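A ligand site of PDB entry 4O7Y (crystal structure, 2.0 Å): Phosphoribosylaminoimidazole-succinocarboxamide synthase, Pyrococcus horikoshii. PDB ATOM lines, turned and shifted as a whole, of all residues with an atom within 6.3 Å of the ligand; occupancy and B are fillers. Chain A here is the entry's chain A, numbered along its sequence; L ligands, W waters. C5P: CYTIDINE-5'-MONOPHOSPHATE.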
ATOM      1  N   GLU A  89      -6.331  -3.537 -22.682  1.00  0.00           N
ATOM      2  CA  GLU A  89      -5.774  -3.035 -21.453  1.00  0.00           C
ATOM      3  C   GLU A  89      -6.029  -1.546 -21.492  1.00  0.00           C
ATOM      4  O   GLU A  89      -5.706  -0.869 -22.488  1.00  0.00           O
ATOM      5  CB  GLU A  89      -4.298  -3.388 -21.348  1.00  0.00           C
ATOM      6  CG  GLU A  89      -4.139  -4.898 -21.176  1.00  0.00           C
ATOM      7  CD  GLU A  89      -2.707  -5.331 -21.050  1.00  0.00           C
ATOM      8  OE1 GLU A  89      -2.407  -6.530 -21.216  1.00  0.00           O
ATOM      9  OE2 GLU A  89      -1.860  -4.463 -20.756  1.00  0.00           O
ATOM     10  N   VAL A  91      -5.520   2.020 -19.858  1.00  0.00           N
ATOM     11  CA  VAL A  91      -4.522   2.647 -18.987  1.00  0.00           C
ATOM     12  C   VAL A  91      -4.939   4.105 -18.711  1.00  0.00           C
ATOM     13  O   VAL A  91      -5.186   4.871 -19.644  1.00  0.00           O
ATOM     14  CB  VAL A  91      -3.112   2.585 -19.626  1.00  0.00           C
ATOM     15  CG1 VAL A  91      -2.095   3.420 -18.834  1.00  0.00           C
ATOM     16  CG2 VAL A  91      -2.609   1.141 -19.744  1.00  0.00           C
ATOM     17  N   VAL A  92      -4.993   4.482 -17.438  1.00  0.00           N
ATOM     18  CA  VAL A  92      -5.339   5.854 -17.035  1.00  0.00           C
ATOM     19  C   VAL A  92      -4.072   6.441 -16.412  1.00  0.00           C
ATOM     20  O   VAL A  92      -3.444   5.793 -15.593  1.00  0.00           O
ATOM     21  CB  VAL A  92      -6.478   5.878 -15.998  1.00  0.00           C
ATOM     22  CG1 VAL A  92      -6.880   7.313 -15.667  1.00  0.00           C
ATOM     23  CG2 VAL A  92      -7.682   5.116 -16.512  1.00  0.00           C
ATOM     24  N   ARG A  93      -3.702   7.656 -16.816  1.00  0.00           N
ATOM     25  CA  ARG A  93      -2.454   8.284 -16.374  1.00  0.00           C
ATOM     26  C   ARG A  93      -2.703   9.696 -15.814  1.00  0.00           C
ATOM     27  O   ARG A  93      -3.361  10.518 -16.460  1.00  0.00           O
ATOM     28  CB  ARG A  93      -1.442   8.294 -17.536  1.00  0.00           C
ATOM     29  CG  ARG A  93      -1.603   7.096 -18.486  1.00  0.00           C
ATOM     30  CD  ARG A  93      -0.531   7.002 -19.570  1.00  0.00           C
ATOM     31  NE  ARG A  93       0.740   6.613 -18.985  1.00  0.00           N
ATOM     32  CZ  ARG A  93       1.425   5.508 -19.244  1.00  0.00           C
ATOM     33  NH1 ARG A  93       1.017   4.613 -20.159  1.00  0.00           N
ATOM     34  NH2 ARG A  93       2.577   5.310 -18.601  1.00  0.00           N
ATOM     35  N   ALA A  97       5.043   9.012 -16.586  1.00  0.00           N
ATOM     36  CA  ALA A  97       5.960   7.930 -16.173  1.00  0.00           C
ATOM     37  C   ALA A  97       5.927   6.848 -17.254  1.00  0.00           C
ATOM     38  O   ALA A  97       5.031   6.849 -18.115  1.00  0.00           O
ATOM     39  CB  ALA A  97       5.523   7.348 -14.824  1.00  0.00           C
ATOM     40  N   GLY A  98       6.890   5.942 -17.214  1.00  0.00           N
ATOM     41  CA  GLY A  98       6.849   4.745 -18.051  1.00  0.00           C
ATOM     42  C   GLY A  98       6.815   5.104 -19.518  1.00  0.00           C
ATOM     43  O   GLY A  98       7.497   6.035 -19.947  1.00  0.00           O
ATOM     44  N   SER A  99       5.984   4.411 -20.267  1.00  0.00           N
ATOM     45  CA  SER A  99       5.939   4.543 -21.727  1.00  0.00           C
ATOM     46  C   SER A  99       5.465   5.924 -22.230  1.00  0.00           C
ATOM     47  O   SER A  99       5.774   6.322 -23.357  1.00  0.00           O
ATOM     48  CB  SER A  99       5.060   3.436 -22.319  1.00  0.00           C
ATOM     49  OG  SER A  99       3.692   3.715 -22.058  1.00  0.00           O
ATOM     50  N   LEU A 100       4.685   6.634 -21.426  1.00  0.00           N
ATOM     51  CA  LEU A 100       4.233   7.989 -21.790  1.00  0.00           C
ATOM     52  C   LEU A 100       5.408   8.949 -22.110  1.00  0.00           C
ATOM     53  O   LEU A 100       5.254   9.851 -22.923  1.00  0.00           O
ATOM     54  CB  LEU A 100       3.300   8.571 -20.703  1.00  0.00           C
ATOM     55  CG  LEU A 100       2.593   9.862 -21.144  1.00  0.00           C
ATOM     56  CD1 LEU A 100       1.837   9.673 -22.468  1.00  0.00           C
ATOM     57  CD2 LEU A 100       1.644  10.327 -20.032  1.00  0.00           C
ATOM     58  N   GLU A 118      -5.496   5.539 -22.235  1.00  0.00           N
ATOM     59  CA  GLU A 118      -4.909   4.887 -23.407  1.00  0.00           C
ATOM     60  C   GLU A 118      -5.484   3.487 -23.535  1.00  0.00           C
ATOM     61  O   GLU A 118      -5.676   2.783 -22.534  1.00  0.00           O
ATOM     62  CB  GLU A 118      -3.381   4.805 -23.324  1.00  0.00           C
ATOM     63  CG  GLU A 118      -2.642   6.132 -23.211  1.00  0.00           C
ATOM     64  CD  GLU A 118      -1.153   5.974 -22.929  1.00  0.00           C
ATOM     65  OE1 GLU A 118      -0.734   4.910 -22.410  1.00  0.00           O
ATOM     66  OE2 GLU A 118      -0.372   6.906 -23.224  1.00  0.00           O
ATOM     67  N   TYR A 120      -4.943  -0.273 -25.227  1.00  0.00           N
ATOM     68  CA  TYR A 120      -3.930  -1.204 -25.751  1.00  0.00           C
ATOM     69  C   TYR A 120      -4.644  -2.493 -26.163  1.00  0.00           C
ATOM     70  O   TYR A 120      -5.477  -3.004 -25.437  1.00  0.00           O
ATOM     71  CB  TYR A 120      -2.825  -1.531 -24.733  1.00  0.00           C
ATOM     72  CG  TYR A 120      -1.945  -0.337 -24.457  1.00  0.00           C
ATOM     73  CD1 TYR A 120      -0.784  -0.126 -25.189  1.00  0.00           C
ATOM     74  CD2 TYR A 120      -2.314   0.599 -23.481  1.00  0.00           C
ATOM     75  CE1 TYR A 120       0.012   1.013 -24.966  1.00  0.00           C
ATOM     76  CE2 TYR A 120      -1.515   1.713 -23.238  1.00  0.00           C
ATOM     77  CZ  TYR A 120      -0.353   1.909 -23.984  1.00  0.00           C
ATOM     78  OH  TYR A 120       0.408   3.039 -23.752  1.00  0.00           O
ATOM     79  N   ASP A 128       0.976  -6.152 -27.577  1.00  0.00           N
ATOM     80  CA  ASP A 128      -0.024  -5.219 -27.032  1.00  0.00           C
ATOM     81  C   ASP A 128       0.085  -3.801 -27.574  1.00  0.00           C
ATOM     82  O   ASP A 128       0.423  -2.905 -26.839  1.00  0.00           O
ATOM     83  CB  ASP A 128       0.075  -5.166 -25.519  1.00  0.00           C
ATOM     84  CG  ASP A 128      -0.062  -6.541 -24.888  1.00  0.00           C
ATOM     85  OD1 ASP A 128      -0.685  -7.444 -25.455  1.00  0.00           O
ATOM     86  OD2 ASP A 128       0.487  -6.699 -23.812  1.00  0.00           O
ATOM     87  N   ASP A 173      -0.350   6.177 -12.316  1.00  0.00           N
ATOM     88  CA  ASP A 173      -1.100   5.620 -13.463  1.00  0.00           C
ATOM     89  C   ASP A 173      -1.565   4.222 -13.080  1.00  0.00           C
ATOM     90  O   ASP A 173      -1.214   3.741 -12.009  1.00  0.00           O
ATOM     91  CB  ASP A 173      -0.283   5.640 -14.781  1.00  0.00           C
ATOM     92  CG  ASP A 173       1.049   4.818 -14.706  1.00  0.00           C
ATOM     93  OD1 ASP A 173       1.139   3.776 -14.035  1.00  0.00           O
ATOM     94  OD2 ASP A 173       2.035   5.215 -15.347  1.00  0.00           O
ATOM     95  N   PHE A 174      -2.355   3.565 -13.924  1.00  0.00           N
ATOM     96  CA  PHE A 174      -2.754   2.186 -13.644  1.00  0.00           C
ATOM     97  C   PHE A 174      -3.428   1.566 -14.856  1.00  0.00           C
ATOM     98  O   PHE A 174      -3.870   2.256 -15.770  1.00  0.00           O
ATOM     99  CB  PHE A 174      -3.686   2.070 -12.414  1.00  0.00           C
ATOM    100  CG  PHE A 174      -4.982   2.815 -12.566  1.00  0.00           C
ATOM    101  CD1 PHE A 174      -6.156   2.139 -12.915  1.00  0.00           C
ATOM    102  CD2 PHE A 174      -5.048   4.188 -12.352  1.00  0.00           C
ATOM    103  CE1 PHE A 174      -7.356   2.825 -13.062  1.00  0.00           C
ATOM    104  CE2 PHE A 174      -6.259   4.872 -12.477  1.00  0.00           C
ATOM    105  CZ  PHE A 174      -7.428   4.186 -12.848  1.00  0.00           C
ATOM    106  N   LYS A 175      -3.526   0.248 -14.843  1.00  0.00           N
ATOM    107  CA  LYS A 175      -4.122  -0.493 -15.929  1.00  0.00           C
ATOM    108  C   LYS A 175      -5.349  -1.261 -15.413  1.00  0.00           C
ATOM    109  O   LYS A 175      -5.299  -1.902 -14.342  1.00  0.00           O
ATOM    110  CB  LYS A 175      -3.116  -1.474 -16.533  1.00  0.00           C
ATOM    111  CG  LYS A 175      -3.631  -2.281 -17.741  1.00  0.00           C
ATOM    112  CD  LYS A 175      -4.319  -3.596 -17.326  1.00  0.00           C
ATOM    113  CE  LYS A 175      -3.330  -4.641 -16.781  1.00  0.00           C
ATOM    114  NZ  LYS A 175      -4.063  -5.837 -16.223  1.00  0.00           N
ATOM    115  N   GLU A 177      -8.808  -3.871 -16.843  1.00  0.00           N
ATOM    116  CA  GLU A 177      -9.381  -4.747 -17.866  1.00  0.00           C
ATOM    117  C   GLU A 177     -10.866  -4.934 -17.593  1.00  0.00           C
ATOM    118  O   GLU A 177     -11.343  -4.771 -16.455  1.00  0.00           O
ATOM    119  CB  GLU A 177      -8.654  -6.096 -17.918  1.00  0.00           C
ATOM    120  CG  GLU A 177      -7.146  -5.988 -18.145  1.00  0.00           C
ATOM    121  CD  GLU A 177      -6.492  -7.327 -18.454  1.00  0.00           C
ATOM    122  OE1 GLU A 177      -7.176  -8.313 -18.792  1.00  0.00           O
ATOM    123  OE2 GLU A 177      -5.277  -7.393 -18.391  1.00  0.00           O
ATOM    124  N   PRO A 194      -0.311  -3.366  -6.684  1.00  0.00           N
ATOM    125  CA  PRO A 194       0.938  -2.663  -6.998  1.00  0.00           C
ATOM    126  C   PRO A 194       1.657  -3.250  -8.248  1.00  0.00           C
ATOM    127  O   PRO A 194       2.648  -2.679  -8.705  1.00  0.00           O
ATOM    128  CB  PRO A 194       1.791  -2.888  -5.739  1.00  0.00           C
ATOM    129  CG  PRO A 194       0.796  -3.191  -4.654  1.00  0.00           C
ATOM    130  CD  PRO A 194      -0.258  -4.002  -5.350  1.00  0.00           C
ATOM    131  N   ASP A 195       1.174  -4.393  -8.755  1.00  0.00           N
ATOM    132  CA  ASP A 195       1.654  -4.920 -10.042  1.00  0.00           C
ATOM    133  C   ASP A 195       1.112  -4.106 -11.215  1.00  0.00           C
ATOM    134  O   ASP A 195       1.828  -3.882 -12.199  1.00  0.00           O
ATOM    135  CB  ASP A 195       1.193  -6.369 -10.250  1.00  0.00           C
ATOM    136  CG  ASP A 195       2.210  -7.410  -9.779  1.00  0.00           C
ATOM    137  OD1 ASP A 195       2.113  -8.554 -10.256  1.00  0.00           O
ATOM    138  OD2 ASP A 195       3.077  -7.128  -8.927  1.00  0.00           O
ATOM    139  N   THR A 196      -0.142  -3.668 -11.090  1.00  0.00           N
ATOM    140  CA  THR A 196      -0.854  -3.028 -12.201  1.00  0.00           C
ATOM    141  C   THR A 196      -1.093  -1.516 -12.042  1.00  0.00           C
ATOM    142  O   THR A 196      -1.815  -0.935 -12.828  1.00  0.00           O
ATOM    143  CB  THR A 196      -2.193  -3.747 -12.477  1.00  0.00           C
ATOM    144  OG1 THR A 196      -3.047  -3.642 -11.336  1.00  0.00           O
ATOM    145  CG2 THR A 196      -1.973  -5.218 -12.818  1.00  0.00           C
ATOM    146  N   CYS A 197      -0.475  -0.908 -11.033  1.00  0.00           N
ATOM    147  CA  CYS A 197      -0.563   0.529 -10.766  1.00  0.00           C
ATOM    148  C   CYS A 197       0.824   1.088 -10.513  1.00  0.00           C
ATOM    149  O   CYS A 197       1.725   0.369 -10.114  1.00  0.00           O
ATOM    150  CB  CYS A 197      -1.419   0.835  -9.532  1.00  0.00           C
ATOM    151  SG  CYS A 197      -3.083   0.110  -9.481  1.00  0.00           S
ATOM    152  N   ARG A 198       0.998   2.374 -10.760  1.00  0.00           N
ATOM    153  CA  ARG A 198       2.136   3.072 -10.173  1.00  0.00           C
ATOM    154  C   ARG A 198       1.675   3.885  -8.989  1.00  0.00           C
ATOM    155  O   ARG A 198       0.742   4.678  -9.115  1.00  0.00           O
ATOM    156  CB  ARG A 198       2.848   3.964 -11.188  1.00  0.00           C
ATOM    157  CG  ARG A 198       3.769   3.177 -12.119  1.00  0.00           C
ATOM    158  CD  ARG A 198       4.566   4.092 -13.039  1.00  0.00           C
ATOM    159  NE  ARG A 198       5.459   3.270 -13.870  1.00  0.00           N
ATOM    160  CZ  ARG A 198       5.201   2.876 -15.108  1.00  0.00           C
ATOM    161  NH1 ARG A 198       4.087   3.258 -15.733  1.00  0.00           N
ATOM    162  NH2 ARG A 198       6.074   2.124 -15.751  1.00  0.00           N
ATOM    163  N   LYS A 210       5.502  -2.202  -8.706  1.00  0.00           N
ATOM    164  CA  LYS A 210       6.305  -3.053  -9.539  1.00  0.00           C
ATOM    165  C   LYS A 210       7.561  -2.398 -10.153  1.00  0.00           C
ATOM    166  O   LYS A 210       8.463  -3.111 -10.548  1.00  0.00           O
ATOM    167  CB  LYS A 210       5.434  -3.719 -10.632  1.00  0.00           C
ATOM    168  CG  LYS A 210       6.115  -4.865 -11.361  1.00  0.00           C
ATOM    169  CD  LYS A 210       5.086  -5.742 -12.069  1.00  0.00           C
ATOM    170  CE  LYS A 210       5.460  -5.904 -13.527  1.00  0.00           C
ATOM    171  NZ  LYS A 210       4.744  -7.020 -14.201  1.00  0.00           N
ATOM    172  N   ASP A 211       7.629  -1.067 -10.206  1.00  0.00           N
ATOM    173  CA  ASP A 211       8.815  -0.366 -10.729  1.00  0.00           C
ATOM    174  C   ASP A 211      10.079  -0.677  -9.870  1.00  0.00           C
ATOM    175  O   ASP A 211      11.198  -0.650 -10.379  1.00  0.00           O
ATOM    176  CB  ASP A 211       8.594   1.140 -10.841  1.00  0.00           C
ATOM    177  CG  ASP A 211       7.829   1.543 -12.113  1.00  0.00           C
ATOM    178  OD1 ASP A 211       7.778   0.777 -13.111  1.00  0.00           O
ATOM    179  OD2 ASP A 211       7.319   2.673 -12.127  1.00  0.00           O
ATOM    180  N   ARG A 214      11.030  -3.689 -11.647  1.00  0.00           N
ATOM    181  CA  ARG A 214      11.421  -3.356 -13.023  1.00  0.00           C
ATOM    182  C   ARG A 214      12.821  -2.739 -13.039  1.00  0.00           C
ATOM    183  O   ARG A 214      13.650  -3.138 -13.856  1.00  0.00           O
ATOM    184  CB  ARG A 214      10.443  -2.385 -13.692  1.00  0.00           C
ATOM    185  CG  ARG A 214       9.189  -3.032 -14.241  1.00  0.00           C
ATOM    186  CD  ARG A 214       8.292  -1.981 -14.904  1.00  0.00           C
ATOM    187  NE  ARG A 214       6.954  -2.531 -15.146  1.00  0.00           N
ATOM    188  CZ  ARG A 214       5.843  -2.168 -14.488  1.00  0.00           C
ATOM    189  NH1 ARG A 214       4.680  -2.757 -14.792  1.00  0.00           N
ATOM    190  NH2 ARG A 214       5.859  -1.224 -13.545  1.00  0.00           N
HETATM  191  O3P C5P L   1       2.511   1.966 -20.427  1.00  0.00           O
HETATM  192  P   C5P L   1       3.392   1.737 -19.205  1.00  0.00           P
HETATM  193  O1P C5P L   1       4.337   0.578 -19.343  1.00  0.00           O
HETATM  194  O2P C5P L   1       4.021   3.017 -18.717  1.00  0.00           O
HETATM  195  O5' C5P L   1       2.454   1.269 -18.017  1.00  0.00           O
HETATM  196  C5' C5P L   1       1.299   2.055 -17.623  1.00  0.00           C
HETATM  197  C4' C5P L   1       0.660   1.478 -16.353  1.00  0.00           C
HETATM  198  O4' C5P L   1      -0.107   0.335 -16.727  1.00  0.00           O
HETATM  199  C3' C5P L   1       1.649   0.977 -15.284  1.00  0.00           C
HETATM  200  O3' C5P L   1       1.067   1.147 -13.989  1.00  0.00           O
HETATM  201  C2' C5P L   1       1.808  -0.498 -15.550  1.00  0.00           C
HETATM  202  O2' C5P L   1       2.113  -1.231 -14.351  1.00  0.00           O
HETATM  203  C1' C5P L   1       0.423  -0.848 -16.086  1.00  0.00           C
HETATM  204  N1  C5P L   1       0.441  -1.962 -17.037  1.00  0.00           N
HETATM  205  C2  C5P L   1      -0.012  -3.265 -16.631  1.00  0.00           C
HETATM  206  N3  C5P L   1       0.006  -4.294 -17.515  1.00  0.00           N
HETATM  207  C4  C5P L   1       0.438  -4.089 -18.771  1.00  0.00           C
HETATM  208  C5  C5P L   1       0.901  -2.836 -19.195  1.00  0.00           C
HETATM  209  C6  C5P L   1       0.891  -1.764 -18.309  1.00  0.00           C
HETATM  210  O2  C5P L   1      -0.433  -3.451 -15.467  1.00  0.00           O
HETATM  211  N4  C5P L   1       0.445  -5.121 -19.648  1.00  0.00           N
HETATM  212  O   HOH W   1       3.227  -1.211 -11.696  1.00  0.00           O
HETATM  213  O   HOH W   2       0.706  -0.082 -21.211  1.00  0.00           O
HETATM  214  O   HOH W   3       1.310  -4.573 -21.971  1.00  0.00           O
HETATM  215  O   HOH W   4      -0.970  -7.239 -17.824  1.00  0.00           O
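OD1 of Asp 173 lies within hydrogen-bond range of O3' of the ligand (2.6 Å). A nitrogen (N4) of the ligand lies within hydrogen-bond range of the side-chain carboxylate (OE2) of Glu 89, 2.6 Å away. An oxygen (O2P) of the ligand is in hydrogen-bond range of the backbone NH (N) of Ser 99 (2.9 Å). An oxygen (O3P) of the ligand is in hydrogen-bond range of the side-chain hydroxyl of Ser 99. The guanidinium group (NH2) of Arg 93 is in salt-bridge range of an oxygen (O2P) of the ligand (2.7 Å). O3' of the ligand lies within hydrogen-bond range of N of Arg 198 (3.5 Å). The guanidinium group (NH1) of Arg 198 lies within salt-bridge range of an oxygen (O2P) of the ligand (3.0 Å). NH1 of Arg 214 sits at hydrogen-bond distance from O2' of the ligand (3.0 Å). An oxygen (O2') of the ligand is in hydrogen-bond range of the backbone carbonyl oxygen (O) of Asp 195 (3.4 Å).
OD2 of Asp 173 is in salt-bridge range of NH1 of Arg 198, 2.9 Å away. The backbone carbonyl oxygen (O) of Glu 89 is in hydrogen-bond range of the backbone NH (N) of Tyr 120, at 2.9 Å. The side-chain hydroxyl (OG) of Ser 99 sits at hydrogen-bond distance from the guanidinium group (NH1) of Arg 93, 3.4 Å away. The guanidinium group (NH2) of Arg 93 lies within hydrogen-bond range of the backbone carbonyl oxygen (O) of Ala 97 (2.9 Å). The guanidinium group of Arg 93 lies within salt-bridge range of the side-chain carboxylate of Glu 118 (2.9 Å). The side-chain carboxylate (OD2) of Asp 211 is in salt-bridge range of the guanidinium group (NE) of Arg 198 (2.6 Å). OE2 of Glu 177 is in salt-bridge range of NZ of Lys 175 (2.9 Å). The backbone NH (N) of Phe 174 lies within hydrogen-bond range of the backbone carbonyl oxygen (O) of Val 92 (3.0 Å).
Val 91 touches the ligand (CG1 to C5', 3.9 Å). CA of Gly 98 touches O2P of the ligand (3.4 Å). Phe 174 touches the ligand. Lys 175 touches the ligand. Thr 196 touches the ligand. Cys 197 touches the ligand (C to O3', 3.5 Å). Hydrophobic or aromatic side chains that line the ligand: Val 91. Within 4 Å of the ligand: Glu 89, Val 91, Arg 93, Gly 98, Ser 99, Asp 173, Phe 174, Lys 175, Asp 195, Thr 196, Cys 197, Arg 198 and Arg 214.
Water W3 lies within hydrogen-bond range of N4 of the ligand, OD2 of Asp 128 and OE2 of Glu 89.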
